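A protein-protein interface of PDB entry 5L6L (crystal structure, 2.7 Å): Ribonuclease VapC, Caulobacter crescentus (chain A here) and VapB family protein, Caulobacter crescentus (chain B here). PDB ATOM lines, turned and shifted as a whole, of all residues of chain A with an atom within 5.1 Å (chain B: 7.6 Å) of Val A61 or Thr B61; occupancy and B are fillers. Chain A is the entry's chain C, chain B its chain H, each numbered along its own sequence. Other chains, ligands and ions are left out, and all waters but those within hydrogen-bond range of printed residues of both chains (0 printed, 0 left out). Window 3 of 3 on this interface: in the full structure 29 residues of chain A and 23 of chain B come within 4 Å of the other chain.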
ATOM      1  N   SER A  57      14.620  14.367 -19.357  1.00  0.00           N
ATOM      2  CA  SER A  57      14.395  15.242 -20.500  1.00  0.00           C
ATOM      3  C   SER A  57      15.024  16.608 -20.276  1.00  0.00           C
ATOM      4  O   SER A  57      15.635  17.170 -21.186  1.00  0.00           O
ATOM      5  CB  SER A  57      12.897  15.371 -20.758  1.00  0.00           C
ATOM      6  OG  SER A  57      12.664  15.614 -22.114  1.00  0.00           O
ATOM      7  N   ARG A  58      14.901  17.164 -19.075  1.00  0.00           N
ATOM      8  CA  ARG A  58      15.469  18.488 -18.886  1.00  0.00           C
ATOM      9  C   ARG A  58      17.001  18.449 -18.910  1.00  0.00           C
ATOM     10  O   ARG A  58      17.634  19.306 -19.536  1.00  0.00           O
ATOM     11  CB  ARG A  58      14.907  19.114 -17.609  1.00  0.00           C
ATOM     12  CG  ARG A  58      13.396  19.232 -17.630  1.00  0.00           C
ATOM     13  CD  ARG A  58      12.833  19.872 -16.377  1.00  0.00           C
ATOM     14  NE  ARG A  58      13.468  21.149 -16.112  1.00  0.00           N
ATOM     15  CZ  ARG A  58      12.938  22.303 -16.463  1.00  0.00           C
ATOM     16  NH1 ARG A  58      11.757  22.328 -17.067  1.00  0.00           N
ATOM     17  NH2 ARG A  58      13.582  23.424 -16.217  1.00  0.00           N
ATOM     18  N   LEU A  59      17.617  17.445 -18.280  1.00  0.00           N
ATOM     19  CA  LEU A  59      19.078  17.322 -18.326  1.00  0.00           C
ATOM     20  C   LEU A  59      19.582  17.121 -19.747  1.00  0.00           C
ATOM     21  O   LEU A  59      20.629  17.669 -20.128  1.00  0.00           O
ATOM     22  CB  LEU A  59      19.562  16.164 -17.457  1.00  0.00           C
ATOM     23  CG  LEU A  59      21.081  15.984 -17.471  1.00  0.00           C
ATOM     24  CD1 LEU A  59      21.844  17.316 -17.147  1.00  0.00           C
ATOM     25  CD2 LEU A  59      21.495  14.849 -16.547  1.00  0.00           C
ATOM     26  N   ASP A  60      18.866  16.322 -20.543  1.00  0.00           N
ATOM     27  CA  ASP A  60      19.306  16.085 -21.906  1.00  0.00           C
ATOM     28  C   ASP A  60      19.389  17.393 -22.676  1.00  0.00           C
ATOM     29  O   ASP A  60      20.401  17.683 -23.332  1.00  0.00           O
ATOM     30  CB  ASP A  60      18.361  15.103 -22.591  1.00  0.00           C
ATOM     31  CG  ASP A  60      18.540  13.676 -22.097  1.00  0.00           C
ATOM     32  OD1 ASP A  60      19.540  13.400 -21.393  1.00  0.00           O
ATOM     33  OD2 ASP A  60      17.683  12.830 -22.422  1.00  0.00           O
ATOM     34  N   VAL A  61      18.341  18.216 -22.576  1.00  0.00           N
ATOM     35  CA  VAL A  61      18.314  19.486 -23.292  1.00  0.00           C
ATOM     36  C   VAL A  61      19.492  20.368 -22.857  1.00  0.00           C
ATOM     37  O   VAL A  61      20.143  21.011 -23.694  1.00  0.00           O
ATOM     38  CB  VAL A  61      16.938  20.176 -23.115  1.00  0.00           C
ATOM     39  CG1 VAL A  61      16.977  21.612 -23.572  1.00  0.00           C
ATOM     40  CG2 VAL A  61      15.865  19.447 -23.874  1.00  0.00           C
ATOM     41  N   MET A  62      19.819  20.381 -21.565  1.00  0.00           N
ATOM     42  CA  MET A  62      20.995  21.135 -21.117  1.00  0.00           C
ATOM     43  C   MET A  62      22.272  20.610 -21.776  1.00  0.00           C
ATOM     44  O   MET A  62      23.102  21.389 -22.266  1.00  0.00           O
ATOM     45  CB  MET A  62      21.143  21.073 -19.609  1.00  0.00           C
ATOM     46  CG  MET A  62      19.995  21.680 -18.855  1.00  0.00           C
ATOM     47  SD  MET A  62      20.129  21.378 -16.928  1.00  0.00           S
ATOM     48  CE  MET A  62      21.954  22.001 -16.599  1.00  0.00           C
ATOM     49  N   LEU A  63      22.416  19.278 -21.802  1.00  0.00           N
ATOM     50  CA  LEU A  63      23.626  18.682 -22.351  1.00  0.00           C
ATOM     51  C   LEU A  63      23.705  18.810 -23.873  1.00  0.00           C
ATOM     52  O   LEU A  63      24.801  18.703 -24.430  1.00  0.00           O
ATOM     53  CB  LEU A  63      23.730  17.220 -21.919  1.00  0.00           C
ATOM     54  CG  LEU A  63      23.886  16.979 -20.416  1.00  0.00           C
ATOM     55  CD1 LEU A  63      23.564  15.551 -20.081  1.00  0.00           C
ATOM     56  CD2 LEU A  63      25.279  17.325 -19.929  1.00  0.00           C
ATOM     57  N   LYS A  64      22.583  19.069 -24.560  1.00  0.00           N
ATOM     58  CA  LYS A  64      22.685  19.398 -25.977  1.00  0.00           C
ATOM     59  C   LYS A  64      23.253  20.797 -26.223  1.00  0.00           C
ATOM     60  O   LYS A  64      23.652  21.084 -27.350  1.00  0.00           O
ATOM     61  CB  LYS A  64      21.316  19.253 -26.667  1.00  0.00           C
ATOM     62  CG  LYS A  64      21.054  17.872 -27.298  1.00  0.00           C
ATOM     63  CD  LYS A  64      19.598  17.641 -27.612  1.00  0.00           C
ATOM     64  CE  LYS A  64      19.071  18.654 -28.652  1.00  0.00           C
ATOM     65  NZ  LYS A  64      17.577  18.597 -28.901  1.00  0.00           N
ATOM     66  N   VAL A  65      23.357  21.655 -25.204  1.00  0.00           N
ATOM     67  CA  VAL A  65      23.691  23.063 -25.391  1.00  0.00           C
ATOM     68  C   VAL A  65      24.963  23.466 -24.649  1.00  0.00           C
ATOM     69  O   VAL A  65      25.813  24.163 -25.214  1.00  0.00           O
ATOM     70  CB  VAL A  65      22.508  23.970 -24.980  1.00  0.00           C
ATOM     71  CG1 VAL A  65      22.906  25.437 -24.972  1.00  0.00           C
ATOM     72  CG2 VAL A  65      21.324  23.735 -25.910  1.00  0.00           C
ATOM     73  N   ALA B  56      19.241  30.328 -24.842  1.00  0.00           N
ATOM     74  CA  ALA B  56      18.048  29.909 -25.574  1.00  0.00           C
ATOM     75  C   ALA B  56      17.574  28.579 -24.972  1.00  0.00           C
ATOM     76  O   ALA B  56      16.389  28.280 -24.944  1.00  0.00           O
ATOM     77  CB  ALA B  56      18.321  29.827 -27.089  1.00  0.00           C
ATOM     78  N   ASP B  57      18.517  27.775 -24.497  1.00  0.00           N
ATOM     79  CA  ASP B  57      18.411  26.768 -23.452  1.00  0.00           C
ATOM     80  C   ASP B  57      17.409  27.122 -22.366  1.00  0.00           C
ATOM     81  O   ASP B  57      16.471  26.368 -22.095  1.00  0.00           O
ATOM     82  CB  ASP B  57      19.801  26.594 -22.845  1.00  0.00           C
ATOM     83  CG  ASP B  57      19.960  25.304 -22.092  1.00  0.00           C
ATOM     84  OD1 ASP B  57      19.400  24.261 -22.532  1.00  0.00           O
ATOM     85  OD2 ASP B  57      20.673  25.348 -21.059  1.00  0.00           O
ATOM     86  N   LEU B  58      17.623  28.256 -21.717  1.00  0.00           N
ATOM     87  CA  LEU B  58      16.672  28.727 -20.724  1.00  0.00           C
ATOM     88  C   LEU B  58      15.258  28.853 -21.300  1.00  0.00           C
ATOM     89  O   LEU B  58      14.266  28.464 -20.669  1.00  0.00           O
ATOM     90  CB  LEU B  58      17.139  30.068 -20.186  1.00  0.00           C
ATOM     91  CG  LEU B  58      15.964  30.441 -19.328  1.00  0.00           C
ATOM     92  CD1 LEU B  58      16.118  29.471 -18.226  1.00  0.00           C
ATOM     93  CD2 LEU B  58      15.927  31.856 -18.833  1.00  0.00           C
ATOM     94  N   VAL B  59      15.143  29.402 -22.495  1.00  0.00           N
ATOM     95  CA  VAL B  59      13.849  29.436 -23.151  1.00  0.00           C
ATOM     96  C   VAL B  59      13.470  28.057 -23.655  1.00  0.00           C
ATOM     97  O   VAL B  59      12.351  27.583 -23.437  1.00  0.00           O
ATOM     98  CB  VAL B  59      13.904  30.441 -24.302  1.00  0.00           C
ATOM     99  CG1 VAL B  59      12.680  31.385 -24.268  1.00  0.00           C
ATOM    100  CG2 VAL B  59      15.242  31.186 -24.221  1.00  0.00           C
ATOM    101  N   ALA B  60      14.412  27.391 -24.317  1.00  0.00           N
ATOM    102  CA  ALA B  60      14.108  26.445 -25.383  1.00  0.00           C
ATOM    103  C   ALA B  60      14.904  25.168 -25.236  1.00  0.00           C
ATOM    104  O   ALA B  60      16.027  25.039 -25.709  1.00  0.00           O
ATOM    105  CB  ALA B  60      14.356  27.088 -26.784  1.00  0.00           C
ATOM    106  N   THR B  61      14.250  24.221 -24.596  1.00  0.00           N
ATOM    107  CA  THR B  61      12.875  24.524 -24.239  1.00  0.00           C
ATOM    108  C   THR B  61      12.657  24.739 -22.764  1.00  0.00           C
ATOM    109  O   THR B  61      11.530  24.599 -22.341  1.00  0.00           O
ATOM    110  CB  THR B  61      11.869  23.398 -24.729  1.00  0.00           C
ATOM    111  OG1 THR B  61      12.587  22.269 -25.257  1.00  0.00           O
ATOM    112  CG2 THR B  61      10.864  23.939 -25.802  1.00  0.00           C
ATOM    113  N   LEU B  62      13.679  25.096 -21.981  1.00  0.00           N
ATOM    114  CA  LEU B  62      13.613  24.759 -20.555  1.00  0.00           C
ATOM    115  C   LEU B  62      12.352  25.313 -19.893  1.00  0.00           C
ATOM    116  O   LEU B  62      11.583  24.565 -19.285  1.00  0.00           O
ATOM    117  CB  LEU B  62      14.878  25.205 -19.818  1.00  0.00           C
ATOM    118  CG  LEU B  62      15.677  24.081 -19.102  1.00  0.00           C
ATOM    119  CD1 LEU B  62      15.801  22.770 -19.885  1.00  0.00           C
ATOM    120  CD2 LEU B  62      17.060  24.556 -18.714  1.00  0.00           C
ATOM    121  N   ASN B  63      12.076  26.601 -20.064  1.00  0.00           N
ATOM    122  CA  ASN B  63      10.872  27.186 -19.480  1.00  0.00           C
ATOM    123  C   ASN B  63       9.584  26.789 -20.193  1.00  0.00           C
ATOM    124  O   ASN B  63       8.499  27.079 -19.669  1.00  0.00           O
ATOM    125  CB  ASN B  63      10.989  28.707 -19.458  1.00  0.00           C
ATOM    126  CG  ASN B  63      11.978  29.201 -18.422  1.00  0.00           C
ATOM    127  OD1 ASN B  63      12.236  28.525 -17.429  1.00  0.00           O
ATOM    128  ND2 ASN B  63      12.538  30.383 -18.650  1.00  0.00           N
ATOM    129  N   GLN B  64       9.659  26.174 -21.375  1.00  0.00           N
ATOM    130  CA  GLN B  64       8.462  25.634 -21.993  1.00  0.00           C
ATOM    131  C   GLN B  64       8.109  24.260 -21.445  1.00  0.00           C
ATOM    132  O   GLN B  64       6.995  23.780 -21.662  1.00  0.00           O
ATOM    133  CB  GLN B  64       8.639  25.572 -23.510  1.00  0.00           C
ATOM    134  CG  GLN B  64       8.762  26.931 -24.175  1.00  0.00           C
ATOM    135  CD  GLN B  64       7.573  27.852 -23.850  1.00  0.00           C
ATOM    136  OE1 GLN B  64       6.431  27.560 -24.213  1.00  0.00           O
ATOM    137  NE2 GLN B  64       7.843  28.957 -23.136  1.00  0.00           N
ATOM    138  N   MET B  65       9.025  23.628 -20.729  1.00  0.00           N
ATOM    139  CA  MET B  65       8.835  22.269 -20.270  1.00  0.00           C
ATOM    140  C   MET B  65       8.392  22.297 -18.838  1.00  0.00           C
ATOM    141  O   MET B  65       8.784  23.200 -18.107  1.00  0.00           O
ATOM    142  CB  MET B  65      10.126  21.472 -20.409  1.00  0.00           C
ATOM    143  CG  MET B  65      10.692  21.472 -21.799  1.00  0.00           C
ATOM    144  SD  MET B  65      12.568  20.940 -21.834  1.00  0.00           S
ATOM    145  CE  MET B  65      12.354  19.055 -21.368  1.00  0.00           C
ATOM    146  N   PRO B  66       7.576  21.330 -18.424  1.00  0.00           N
ATOM    147  CA  PRO B  66       7.210  21.262 -17.018  1.00  0.00           C
ATOM    148  C   PRO B  66       8.464  21.226 -16.161  1.00  0.00           C
ATOM    149  O   PRO B  66       9.550  20.872 -16.622  1.00  0.00           O
ATOM    150  CB  PRO B  66       6.414  19.955 -16.924  1.00  0.00           C
ATOM    151  CG  PRO B  66       5.962  19.686 -18.265  1.00  0.00           C
ATOM    152  CD  PRO B  66       7.012  20.198 -19.168  1.00  0.00           C
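OG1 of Thr B61 lies within hydrogen-bond range of SD of Met B65, at 3.7 Å. O of Asp B57 sits close to N of Leu B62 (3.1 Å).
Val A61 touches just these residues of chain B: Asp B57 and Thr B61. Printed residues of chain B within 4 Å of Val A65: Asp B57. Printed residues of chain A within 4 Å of Asp B57: Val A61 (3.5 Å), Met A62 (3.8 Å) and Val A65 (3.9 Å). Val B59 touches none of the printed residues of chain A. Ala B60 touches none of the printed residues of chain A. Thr B61 touches just one residue of chain A: Val A61. Printed residues of chain A within 4 Å of Leu B62: Arg A58. Of the printed residues of chain A, Met B65 touches Ser A57 (3.5 Å) and Arg A58 (3.3 Å). Of the printed residues of chain A, Pro B66 touches Arg A58 (2.7 Å). The nearest printed residue of chain A that does not touch Thr B61 is Arg A58 (5.7 Å). The nearest printed residue of chain A that does not touch Met B65 is Val A61 (4.2 Å).
The backbone carbonyl oxygen (O) of Pro B66 lies within hydrogen-bond range of the guanidinium group (NH1) of Arg A58 (2.7 Å). The guanidinium group (NH1) of Arg A58 is in hydrogen-bond range of the backbone carbonyl oxygen (O) of Leu B62. The backbone carbonyl oxygen (O) of Met B65 is in hydrogen-bond range of the guanidinium group (NH1) of Arg A58, at 3.3 Å.
Among the printed residues, no Asp or Glu carboxylate lies within 4 Å of a Lys or Arg side-chain nitrogen of the other chain.
Among the printed residues, merely in contact across the chains: Val A61 with Asp B57, Ser A57 with Met B65, Met A62 with Asp B57, Val A61 with Thr B61 and Val A65 with Asp B57.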
